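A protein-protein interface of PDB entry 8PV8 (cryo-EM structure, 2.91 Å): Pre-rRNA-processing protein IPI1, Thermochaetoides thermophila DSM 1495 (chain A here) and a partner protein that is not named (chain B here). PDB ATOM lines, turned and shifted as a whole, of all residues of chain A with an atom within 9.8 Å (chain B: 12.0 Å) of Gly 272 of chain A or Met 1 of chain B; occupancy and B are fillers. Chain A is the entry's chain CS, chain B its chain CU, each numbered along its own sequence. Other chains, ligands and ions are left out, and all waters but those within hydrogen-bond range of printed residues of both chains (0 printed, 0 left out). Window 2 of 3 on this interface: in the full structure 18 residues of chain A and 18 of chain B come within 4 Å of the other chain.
Printed residues of chain B within 4 Å of Phe 265 of chain A: Thr 293. Leu 268 of chain A touches none of the printed residues of chain B. No residue of chain B comes within 4 Å of Asn 269 of chain A. Phe 271 of chain A touches just these residues of chain B: Leu 2, Glu 4, Ser 33 and Pro 333. Of chain B, only Met 1 comes within 4 Å of Gly 272 of chain A. Leu 273 of chain A touches none of the printed residues of chain B. No residue of chain B comes within 4 Å of Pro 274 of chain A. Met 1 of chain B touches two residues of chain A. Of chain A, only Leu 270 and Phe 271 come within 4 Å of Leu 2 of chain B. Printed residues of chain A within 4 Å of Glu 4 of chain B: Phe 271 (3.7 Å). Thr 31 of chain B touches none of the printed residues of chain A. Of the printed residues of chain A, Ser 33 of chain B touches Phe 271. Printed residues of chain A within 4 Å of Thr 293 of chain B: Phe 265 (3.8 Å). Of the printed residues of chain A, Pro 333 of chain B touches Phe 271 (3.7 Å).
CE2 of Phe 265 of chain A touches CG2 of Thr 293 of chain B, 3.8 Å away. C of Met 1 of chain B touches O of Leu 270 of chain A, 3.7 Å away. Leu 2 of chain B touches Phe 271 of chain A. CE1 of Phe 271 of chain A touches OE1 of Glu 4 of chain B, 3.7 Å away. CD1 of Phe 271 of chain A touches OG of Ser 33 of chain B, at 3.7 Å. Phe 271 of chain A touches Pro 333 of chain B (CE1 to CG, 3.7 Å). Gly 272 of chain A touches Met 1 of chain B (O to CB, 3.3 Å).
N of Leu 2 of chain B lies within hydrogen-bond range of O of Leu 270 of chain A (2.8 Å).
The backbone carbonyl oxygen (O) of Glu 4 of chain B is in hydrogen-bond range of the backbone NH (N) of Leu 32 of chain B (2.7 Å). OG of Ser 33 of chain B is in hydrogen-bond range of N of Glu 4 of chain B (3.2 Å). The backbone NH (N) of Tyr 290 of chain B is in hydrogen-bond range of the side-chain carboxylate (OE2) of Glu 4 of chain B (2.7 Å). The side-chain carboxylate (OD2) of Asp 291 of chain B sits at hydrogen-bond distance from the side-chain hydroxyl (OG1) of Thr 293 of chain B.
Hydrophobic or aromatic side chains of chain A that line the printed part of chain B: Phe 265, Leu 270 and Phe 271. Printed residues of chain B that touch a printed residue of chain A: Met 1, Leu 2, Glu 4, Ser 33, Thr 293 and Pro 333. Among the printed residues, 8 pairs touch across the chains.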
ATOM      1  N   PRO A 177      -0.805  39.238   5.808  1.00  0.00           N
ATOM      2  CA  PRO A 177      -0.185  38.067   5.166  1.00  0.00           C
ATOM      3  C   PRO A 177      -0.286  38.076   3.649  1.00  0.00           C
ATOM      4  O   PRO A 177      -1.385  38.069   3.086  1.00  0.00           O
ATOM      5  CB  PRO A 177      -0.966  36.891   5.765  1.00  0.00           C
ATOM      6  CG  PRO A 177      -1.407  37.385   7.089  1.00  0.00           C
ATOM      7  CD  PRO A 177      -1.728  38.837   6.886  1.00  0.00           C
ATOM      8  N   PHE A 265      -4.891  37.988  16.470  1.00  0.00           N
ATOM      9  CA  PHE A 265      -4.372  36.622  16.407  1.00  0.00           C
ATOM     10  C   PHE A 265      -4.108  36.154  14.982  1.00  0.00           C
ATOM     11  O   PHE A 265      -4.155  34.952  14.706  1.00  0.00           O
ATOM     12  CB  PHE A 265      -5.298  35.628  17.117  1.00  0.00           C
ATOM     13  CG  PHE A 265      -5.722  36.072  18.483  1.00  0.00           C
ATOM     14  CD1 PHE A 265      -4.795  36.196  19.501  1.00  0.00           C
ATOM     15  CD2 PHE A 265      -7.049  36.363  18.749  1.00  0.00           C
ATOM     16  CE1 PHE A 265      -5.182  36.606  20.758  1.00  0.00           C
ATOM     17  CE2 PHE A 265      -7.442  36.772  20.006  1.00  0.00           C
ATOM     18  CZ  PHE A 265      -6.507  36.894  21.011  1.00  0.00           C
ATOM     19  N   ALA A 266      -3.831  37.082  14.063  1.00  0.00           N
ATOM     20  CA  ALA A 266      -3.473  36.691  12.705  1.00  0.00           C
ATOM     21  C   ALA A 266      -2.062  36.127  12.646  1.00  0.00           C
ATOM     22  O   ALA A 266      -1.761  35.299  11.778  1.00  0.00           O
ATOM     23  CB  ALA A 266      -3.611  37.881  11.758  1.00  0.00           C
ATOM     24  N   TYR A 267      -1.188  36.559  13.555  1.00  0.00           N
ATOM     25  CA  TYR A 267       0.174  36.043  13.588  1.00  0.00           C
ATOM     26  C   TYR A 267       0.232  34.616  14.114  1.00  0.00           C
ATOM     27  O   TYR A 267       1.234  33.927  13.895  1.00  0.00           O
ATOM     28  CB  TYR A 267       1.074  36.956  14.431  1.00  0.00           C
ATOM     29  CG  TYR A 267       0.659  37.131  15.880  1.00  0.00           C
ATOM     30  CD1 TYR A 267      -0.351  38.017  16.239  1.00  0.00           C
ATOM     31  CD2 TYR A 267       1.295  36.422  16.890  1.00  0.00           C
ATOM     32  CE1 TYR A 267      -0.726  38.176  17.559  1.00  0.00           C
ATOM     33  CE2 TYR A 267       0.930  36.579  18.213  1.00  0.00           C
ATOM     34  CZ  TYR A 267      -0.081  37.455  18.540  1.00  0.00           C
ATOM     35  OH  TYR A 267      -0.446  37.612  19.857  1.00  0.00           O
ATOM     36  N   LEU A 268      -0.815  34.157  14.804  1.00  0.00           N
ATOM     37  CA  LEU A 268      -0.865  32.769  15.244  1.00  0.00           C
ATOM     38  C   LEU A 268      -1.141  31.816  14.087  1.00  0.00           C
ATOM     39  O   LEU A 268      -0.473  30.785  13.968  1.00  0.00           O
ATOM     40  CB  LEU A 268      -1.925  32.597  16.330  1.00  0.00           C
ATOM     41  CG  LEU A 268      -1.783  33.479  17.565  1.00  0.00           C
ATOM     42  CD1 LEU A 268      -2.879  33.177  18.567  1.00  0.00           C
ATOM     43  CD2 LEU A 268      -0.428  33.257  18.181  1.00  0.00           C
ATOM     44  N   ASN A 269      -2.114  32.157  13.232  1.00  0.00           N
ATOM     45  CA  ASN A 269      -2.560  31.313  12.115  1.00  0.00           C
ATOM     46  C   ASN A 269      -2.947  29.912  12.588  1.00  0.00           C
ATOM     47  O   ASN A 269      -2.588  28.904  11.977  1.00  0.00           O
ATOM     48  CB  ASN A 269      -1.505  31.243  11.006  1.00  0.00           C
ATOM     49  CG  ASN A 269      -2.086  30.811   9.675  1.00  0.00           C
ATOM     50  OD1 ASN A 269      -3.232  31.126   9.351  1.00  0.00           O
ATOM     51  ND2 ASN A 269      -1.307  30.061   8.907  1.00  0.00           N
ATOM     52  N   LEU A 270      -3.667  29.847  13.710  1.00  0.00           N
ATOM     53  CA  LEU A 270      -4.064  28.553  14.252  1.00  0.00           C
ATOM     54  C   LEU A 270      -5.153  27.905  13.406  1.00  0.00           C
ATOM     55  O   LEU A 270      -5.143  26.687  13.198  1.00  0.00           O
ATOM     56  CB  LEU A 270      -4.535  28.714  15.696  1.00  0.00           C
ATOM     57  CG  LEU A 270      -3.501  29.259  16.681  1.00  0.00           C
ATOM     58  CD1 LEU A 270      -4.147  29.549  18.018  1.00  0.00           C
ATOM     59  CD2 LEU A 270      -2.349  28.285  16.842  1.00  0.00           C
ATOM     60  N   PHE A 271      -6.096  28.702  12.908  1.00  0.00           N
ATOM     61  CA  PHE A 271      -7.258  28.192  12.199  1.00  0.00           C
ATOM     62  C   PHE A 271      -7.126  28.304  10.686  1.00  0.00           C
ATOM     63  O   PHE A 271      -8.079  27.988   9.967  1.00  0.00           O
ATOM     64  CB  PHE A 271      -8.514  28.922  12.671  1.00  0.00           C
ATOM     65  CG  PHE A 271      -8.879  28.629  14.095  1.00  0.00           C
ATOM     66  CD1 PHE A 271      -9.546  27.463  14.426  1.00  0.00           C
ATOM     67  CD2 PHE A 271      -8.545  29.517  15.103  1.00  0.00           C
ATOM     68  CE1 PHE A 271      -9.881  27.191  15.738  1.00  0.00           C
ATOM     69  CE2 PHE A 271      -8.876  29.251  16.417  1.00  0.00           C
ATOM     70  CZ  PHE A 271      -9.546  28.087  16.735  1.00  0.00           C
ATOM     71  N   GLY A 272      -5.972  28.744  10.186  1.00  0.00           N
ATOM     72  CA  GLY A 272      -5.748  28.898   8.768  1.00  0.00           C
ATOM     73  C   GLY A 272      -4.751  27.889   8.218  1.00  0.00           C
ATOM     74  O   GLY A 272      -4.167  27.078   8.932  1.00  0.00           O
ATOM     75  N   LEU A 273      -4.574  27.961   6.903  1.00  0.00           N
ATOM     76  CA  LEU A 273      -3.618  27.116   6.210  1.00  0.00           C
ATOM     77  C   LEU A 273      -2.193  27.540   6.554  1.00  0.00           C
ATOM     78  O   LEU A 273      -1.949  28.699   6.901  1.00  0.00           O
ATOM     79  CB  LEU A 273      -3.839  27.184   4.698  1.00  0.00           C
ATOM     80  CG  LEU A 273      -3.456  28.419   3.868  1.00  0.00           C
ATOM     81  CD1 LEU A 273      -3.435  28.047   2.394  1.00  0.00           C
ATOM     82  CD2 LEU A 273      -4.390  29.606   4.081  1.00  0.00           C
ATOM     83  N   PRO A 274      -1.240  26.606   6.508  1.00  0.00           N
ATOM     84  CA  PRO A 274       0.167  26.978   6.706  1.00  0.00           C
ATOM     85  C   PRO A 274       0.646  27.944   5.633  1.00  0.00           C
ATOM     86  O   PRO A 274       0.249  27.859   4.469  1.00  0.00           O
ATOM     87  CB  PRO A 274       0.904  25.636   6.624  1.00  0.00           C
ATOM     88  CG  PRO A 274      -0.117  24.627   7.013  1.00  0.00           C
ATOM     89  CD  PRO A 274      -1.424  25.144   6.485  1.00  0.00           C
ATOM     90  N   ARG A 275       1.508  28.870   6.038  1.00  0.00           N
ATOM     91  CA  ARG A 275       1.962  29.958   5.184  1.00  0.00           C
ATOM     92  C   ARG A 275       3.399  29.713   4.749  1.00  0.00           C
ATOM     93  O   ARG A 275       4.256  29.383   5.575  1.00  0.00           O
ATOM     94  CB  ARG A 275       1.854  31.300   5.911  1.00  0.00           C
ATOM     95  CG  ARG A 275       0.489  31.562   6.522  1.00  0.00           C
ATOM     96  CD  ARG A 275       0.130  33.035   6.477  1.00  0.00           C
ATOM     97  NE  ARG A 275       0.717  33.772   7.590  1.00  0.00           N
ATOM     98  CZ  ARG A 275       0.055  34.135   8.680  1.00  0.00           C
ATOM     99  NH1 ARG A 275      -1.228  33.856   8.834  1.00  0.00           N
ATOM    100  NH2 ARG A 275       0.697  34.796   9.639  1.00  0.00           N
ATOM    101  N   SER A 279       3.503  34.161   1.480  1.00  0.00           N
ATOM    102  CA  SER A 279       2.270  34.492   2.180  1.00  0.00           C
ATOM    103  C   SER A 279       2.480  34.819   3.652  1.00  0.00           C
ATOM    104  O   SER A 279       1.505  35.140   4.339  1.00  0.00           O
ATOM    105  CB  SER A 279       1.265  33.342   2.053  1.00  0.00           C
ATOM    106  OG  SER A 279       1.754  32.168   2.675  1.00  0.00           O
ATOM    107  N   MET B   1      -3.525  23.041  11.087  1.00  0.00           N
ATOM    108  CA  MET B   1      -4.688  23.879  10.828  1.00  0.00           C
ATOM    109  C   MET B   1      -5.889  23.414  11.643  1.00  0.00           C
ATOM    110  O   MET B   1      -6.528  22.417  11.308  1.00  0.00           O
ATOM    111  CB  MET B   1      -5.032  23.877   9.338  1.00  0.00           C
ATOM    112  N   LEU B   2      -6.184  24.139  12.720  1.00  0.00           N
ATOM    113  CA  LEU B   2      -7.330  23.804  13.554  1.00  0.00           C
ATOM    114  C   LEU B   2      -8.630  24.132  12.833  1.00  0.00           C
ATOM    115  O   LEU B   2      -8.739  25.147  12.139  1.00  0.00           O
ATOM    116  CB  LEU B   2      -7.260  24.563  14.878  1.00  0.00           C
ATOM    117  CG  LEU B   2      -5.974  24.402  15.687  1.00  0.00           C
ATOM    118  CD1 LEU B   2      -5.975  25.359  16.864  1.00  0.00           C
ATOM    119  CD2 LEU B   2      -5.817  22.968  16.157  1.00  0.00           C
ATOM    120  N   THR B   3      -9.623  23.264  13.002  1.00  0.00           N
ATOM    121  CA  THR B   3     -10.933  23.429  12.389  1.00  0.00           C
ATOM    122  C   THR B   3     -11.949  23.740  13.477  1.00  0.00           C
ATOM    123  O   THR B   3     -12.070  22.990  14.450  1.00  0.00           O
ATOM    124  CB  THR B   3     -11.343  22.171  11.617  1.00  0.00           C
ATOM    125  OG1 THR B   3     -10.461  21.985  10.503  1.00  0.00           O
ATOM    126  CG2 THR B   3     -12.771  22.292  11.107  1.00  0.00           C
ATOM    127  N   GLU B   4     -12.675  24.842  13.311  1.00  0.00           N
ATOM    128  CA  GLU B   4     -13.675  25.278  14.274  1.00  0.00           C
ATOM    129  C   GLU B   4     -15.059  24.924  13.749  1.00  0.00           C
ATOM    130  O   GLU B   4     -15.405  25.269  12.615  1.00  0.00           O
ATOM    131  CB  GLU B   4     -13.569  26.781  14.533  1.00  0.00           C
ATOM    132  CG  GLU B   4     -14.310  27.239  15.773  1.00  0.00           C
ATOM    133  CD  GLU B   4     -13.816  28.575  16.283  1.00  0.00           C
ATOM    134  OE1 GLU B   4     -12.971  29.198  15.608  1.00  0.00           O
ATOM    135  OE2 GLU B   4     -14.264  28.996  17.368  1.00  0.00           O
ATOM    136  N   GLU B   5     -15.844  24.239  14.577  1.00  0.00           N
ATOM    137  CA  GLU B   5     -17.134  23.706  14.169  1.00  0.00           C
ATOM    138  C   GLU B   5     -18.216  24.187  15.124  1.00  0.00           C
ATOM    139  O   GLU B   5     -17.958  24.439  16.304  1.00  0.00           O
ATOM    140  CB  GLU B   5     -17.112  22.174  14.142  1.00  0.00           C
ATOM    141  CG  GLU B   5     -16.205  21.589  13.077  1.00  0.00           C
ATOM    142  CD  GLU B   5     -16.150  20.077  13.130  1.00  0.00           C
ATOM    143  OE1 GLU B   5     -16.707  19.493  14.083  1.00  0.00           O
ATOM    144  OE2 GLU B   5     -15.533  19.471  12.228  1.00  0.00           O
ATOM    145  N   THR B  31     -18.969  23.583   9.665  1.00  0.00           N
ATOM    146  CA  THR B  31     -17.613  24.070   9.893  1.00  0.00           C
ATOM    147  C   THR B  31     -17.624  25.585   9.759  1.00  0.00           C
ATOM    148  O   THR B  31     -18.226  26.122   8.822  1.00  0.00           O
ATOM    149  CB  THR B  31     -16.615  23.477   8.898  1.00  0.00           C
ATOM    150  OG1 THR B  31     -17.025  23.792   7.561  1.00  0.00           O
ATOM    151  CG2 THR B  31     -16.501  21.985   9.061  1.00  0.00           C
ATOM    152  N   LEU B  32     -16.962  26.273  10.688  1.00  0.00           N
ATOM    153  CA  LEU B  32     -16.883  27.726  10.593  1.00  0.00           C
ATOM    154  C   LEU B  32     -15.599  28.167   9.900  1.00  0.00           C
ATOM    155  O   LEU B  32     -15.613  29.102   9.092  1.00  0.00           O
ATOM    156  CB  LEU B  32     -16.989  28.349  11.982  1.00  0.00           C
ATOM    157  CG  LEU B  32     -17.045  29.874  12.011  1.00  0.00           C
ATOM    158  CD1 LEU B  32     -18.304  30.388  11.334  1.00  0.00           C
ATOM    159  CD2 LEU B  32     -16.985  30.341  13.439  1.00  0.00           C
ATOM    160  N   SER B  33     -14.483  27.503  10.195  1.00  0.00           N
ATOM    161  CA  SER B  33     -13.194  27.841   9.614  1.00  0.00           C
ATOM    162  C   SER B  33     -12.597  26.587   8.986  1.00  0.00           C
ATOM    163  O   SER B  33     -12.784  25.481   9.521  1.00  0.00           O
ATOM    164  CB  SER B  33     -12.252  28.414  10.681  1.00  0.00           C
ATOM    165  OG  SER B  33     -11.845  27.405  11.586  1.00  0.00           O
ATOM    166  N   PRO B  34     -11.868  26.704   7.862  1.00  0.00           N
ATOM    167  CA  PRO B  34     -11.560  27.937   7.125  1.00  0.00           C
ATOM    168  C   PRO B  34     -12.679  28.393   6.189  1.00  0.00           C
ATOM    169  O   PRO B  34     -12.748  29.576   5.852  1.00  0.00           O
ATOM    170  CB  PRO B  34     -10.313  27.558   6.326  1.00  0.00           C
ATOM    171  CG  PRO B  34     -10.445  26.097   6.100  1.00  0.00           C
ATOM    172  CD  PRO B  34     -11.209  25.527   7.267  1.00  0.00           C
ATOM    173  N   SER B  35     -13.540  27.468   5.777  1.00  0.00           N
ATOM    174  CA  SER B  35     -14.647  27.762   4.878  1.00  0.00           C
ATOM    175  C   SER B  35     -15.929  27.187   5.458  1.00  0.00           C
ATOM    176  O   SER B  35     -15.901  26.138   6.112  1.00  0.00           O
ATOM    177  CB  SER B  35     -14.391  27.189   3.482  1.00  0.00           C
ATOM    178  OG  SER B  35     -14.199  25.787   3.535  1.00  0.00           O
ATOM    179  N   TYR B  36     -17.043  27.873   5.224  1.00  0.00           N
ATOM    180  CA  TYR B  36     -18.327  27.376   5.699  1.00  0.00           C
ATOM    181  C   TYR B  36     -18.766  26.174   4.872  1.00  0.00           C
ATOM    182  O   TYR B  36     -18.749  26.204   3.638  1.00  0.00           O
ATOM    183  CB  TYR B  36     -19.382  28.485   5.640  1.00  0.00           C
ATOM    184  CG  TYR B  36     -20.766  28.050   6.079  1.00  0.00           C
ATOM    185  CD1 TYR B  36     -21.130  28.083   7.418  1.00  0.00           C
ATOM    186  CD2 TYR B  36     -21.717  27.634   5.153  1.00  0.00           C
ATOM    187  CE1 TYR B  36     -22.390  27.693   7.826  1.00  0.00           C
ATOM    188  CE2 TYR B  36     -22.975  27.238   5.551  1.00  0.00           C
ATOM    189  CZ  TYR B  36     -23.308  27.272   6.888  1.00  0.00           C
ATOM    190  OH  TYR B  36     -24.565  26.887   7.285  1.00  0.00           O
ATOM    191  N   LYS B  39     -21.290  19.722   7.404  1.00  0.00           N
ATOM    192  CA  LYS B  39     -20.772  18.362   7.514  1.00  0.00           C
ATOM    193  C   LYS B  39     -21.897  17.343   7.578  1.00  0.00           C
ATOM    194  O   LYS B  39     -22.020  16.486   6.694  1.00  0.00           O
ATOM    195  CB  LYS B  39     -19.884  18.207   8.747  1.00  0.00           C
ATOM    196  CG  LYS B  39     -18.566  18.927   8.700  1.00  0.00           C
ATOM    197  CD  LYS B  39     -17.873  18.789  10.041  1.00  0.00           C
ATOM    198  CE  LYS B  39     -17.390  17.368  10.266  1.00  0.00           C
ATOM    199  NZ  LYS B  39     -16.609  17.248  11.526  1.00  0.00           N
ATOM    200  N   TYR B 290     -14.237  30.218  19.825  1.00  0.00           N
ATOM    201  CA  TYR B 290     -13.214  29.790  20.775  1.00  0.00           C
ATOM    202  C   TYR B 290     -12.229  30.912  21.085  1.00  0.00           C
ATOM    203  O   TYR B 290     -11.864  31.124  22.247  1.00  0.00           O
ATOM    204  CB  TYR B 290     -12.481  28.566  20.226  1.00  0.00           C
ATOM    205  CG  TYR B 290     -11.555  27.882  21.207  1.00  0.00           C
ATOM    206  CD1 TYR B 290     -10.201  28.185  21.242  1.00  0.00           C
ATOM    207  CD2 TYR B 290     -12.035  26.927  22.093  1.00  0.00           C
ATOM    208  CE1 TYR B 290      -9.352  27.559  22.133  1.00  0.00           C
ATOM    209  CE2 TYR B 290     -11.193  26.295  22.986  1.00  0.00           C
ATOM    210  CZ  TYR B 290      -9.854  26.616  23.003  1.00  0.00           C
ATOM    211  OH  TYR B 290      -9.011  25.989  23.891  1.00  0.00           O
ATOM    212  N   ASP B 291     -11.788  31.643  20.060  1.00  0.00           N
ATOM    213  CA  ASP B 291     -10.889  32.766  20.295  1.00  0.00           C
ATOM    214  C   ASP B 291     -11.635  33.960  20.879  1.00  0.00           C
ATOM    215  O   ASP B 291     -11.028  34.835  21.506  1.00  0.00           O
ATOM    216  CB  ASP B 291     -10.169  33.144  18.998  1.00  0.00           C
ATOM    217  CG  ASP B 291     -11.127  33.442  17.849  1.00  0.00           C
ATOM    218  OD1 ASP B 291     -12.357  33.296  18.016  1.00  0.00           O
ATOM    219  OD2 ASP B 291     -10.640  33.827  16.765  1.00  0.00           O
ATOM    220  N   THR B 293     -13.171  36.248  19.091  1.00  0.00           N
ATOM    221  CA  THR B 293     -13.174  37.392  18.188  1.00  0.00           C
ATOM    222  C   THR B 293     -14.442  37.430  17.346  1.00  0.00           C
ATOM    223  O   THR B 293     -14.789  38.474  16.783  1.00  0.00           O
ATOM    224  CB  THR B 293     -11.941  37.347  17.290  1.00  0.00           C
ATOM    225  OG1 THR B 293     -12.014  36.196  16.441  1.00  0.00           O
ATOM    226  CG2 THR B 293     -10.685  37.258  18.132  1.00  0.00           C
ATOM    227  N   MET B 294     -15.145  36.305  17.244  1.00  0.00           N
ATOM    228  CA  MET B 294     -16.280  36.178  16.344  1.00  0.00           C
ATOM    229  C   MET B 294     -17.500  35.635  17.075  1.00  0.00           C
ATOM    230  O   MET B 294     -17.378  34.883  18.047  1.00  0.00           O
ATOM    231  CB  MET B 294     -15.930  35.289  15.143  1.00  0.00           C
ATOM    232  CG  MET B 294     -14.763  35.830  14.315  1.00  0.00           C
ATOM    233  SD  MET B 294     -13.813  34.597  13.411  1.00  0.00           S
ATOM    234  CE  MET B 294     -15.093  33.416  13.031  1.00  0.00           C
ATOM    235  N   ARG B 306     -22.574  35.973  11.022  1.00  0.00           N
ATOM    236  CA  ARG B 306     -21.306  36.057  11.729  1.00  0.00           C
ATOM    237  C   ARG B 306     -20.985  37.514  12.027  1.00  0.00           C
ATOM    238  O   ARG B 306     -21.113  38.375  11.147  1.00  0.00           O
ATOM    239  CB  ARG B 306     -20.179  35.433  10.904  1.00  0.00           C
ATOM    240  CG  ARG B 306     -18.851  35.355  11.632  1.00  0.00           C
ATOM    241  CD  ARG B 306     -17.743  34.830  10.728  1.00  0.00           C
ATOM    242  NE  ARG B 306     -17.642  35.587   9.485  1.00  0.00           N
ATOM    243  CZ  ARG B 306     -16.810  35.295   8.493  1.00  0.00           C
ATOM    244  NH1 ARG B 306     -15.977  34.270   8.569  1.00  0.00           N
ATOM    245  NH2 ARG B 306     -16.813  36.051   7.400  1.00  0.00           N
ATOM    246  N   VAL B 331     -18.126  23.881  19.194  1.00  0.00           N
ATOM    247  CA  VAL B 331     -17.341  22.721  19.593  1.00  0.00           C
ATOM    248  C   VAL B 331     -15.878  23.140  19.630  1.00  0.00           C
ATOM    249  O   VAL B 331     -15.403  23.835  18.726  1.00  0.00           O
ATOM    250  CB  VAL B 331     -17.550  21.529  18.635  1.00  0.00           C
ATOM    251  CG1 VAL B 331     -16.862  20.281  19.166  1.00  0.00           C
ATOM    252  CG2 VAL B 331     -19.031  21.268  18.425  1.00  0.00           C
ATOM    253  N   SER B 332     -15.176  22.738  20.687  1.00  0.00           N
ATOM    254  CA  SER B 332     -13.781  23.119  20.847  1.00  0.00           C
ATOM    255  C   SER B 332     -12.922  22.457  19.771  1.00  0.00           C
ATOM    256  O   SER B 332     -13.108  21.271  19.471  1.00  0.00           O
ATOM    257  CB  SER B 332     -13.275  22.726  22.233  1.00  0.00           C
ATOM    258  OG  SER B 332     -13.275  21.317  22.392  1.00  0.00           O
ATOM    259  N   PRO B 333     -11.980  23.189  19.168  1.00  0.00           N
ATOM    260  CA  PRO B 333     -11.132  22.588  18.126  1.00  0.00           C
ATOM    261  C   PRO B 333     -10.116  21.594  18.658  1.00  0.00           C
ATOM    262  O   PRO B 333      -9.535  20.849  17.859  1.00  0.00           O
ATOM    263  CB  PRO B 333     -10.438  23.802  17.500  1.00  0.00           C
ATOM    264  CG  PRO B 333     -10.413  24.811  18.586  1.00  0.00           C
ATOM    265  CD  PRO B 333     -11.687  24.618  19.359  1.00  0.00           C
ATOM    266  N   PHE B 334      -9.882  21.557  19.965  1.00  0.00           N
ATOM    267  CA  PHE B 334      -8.961  20.611  20.571  1.00  0.00           C
ATOM    268  C   PHE B 334      -9.738  19.431  21.135  1.00  0.00           C
ATOM    269  O   PHE B 334     -10.859  19.576  21.630  1.00  0.00           O
ATOM    270  CB  PHE B 334      -8.140  21.266  21.687  1.00  0.00           C
ATOM    271  CG  PHE B 334      -7.267  22.392  21.219  1.00  0.00           C
ATOM    272  CD1 PHE B 334      -6.081  22.138  20.554  1.00  0.00           C
ATOM    273  CD2 PHE B 334      -7.630  23.706  21.456  1.00  0.00           C
ATOM    274  CE1 PHE B 334      -5.277  23.175  20.128  1.00  0.00           C
ATOM    275  CE2 PHE B 334      -6.830  24.746  21.033  1.00  0.00           C
ATOM    276  CZ  PHE B 334      -5.651  24.480  20.368  1.00  0.00           C
ATOM    277  N   LEU B 335      -9.129  18.253  21.053  1.00  0.00           N
ATOM    278  CA  LEU B 335      -9.704  17.055  21.644  1.00  0.00           C
ATOM    279  C   LEU B 335      -9.332  16.987  23.118  1.00  0.00           C
ATOM    280  O   LEU B 335      -8.210  17.326  23.507  1.00  0.00           O
ATOM    281  CB  LEU B 335      -9.235  15.790  20.912  1.00  0.00           C
ATOM    282  CG  LEU B 335      -7.812  15.227  21.037  1.00  0.00           C
ATOM    283  CD1 LEU B 335      -7.780  13.801  20.515  1.00  0.00           C
ATOM    284  CD2 LEU B 335      -6.777  16.071  20.301  1.00  0.00           C
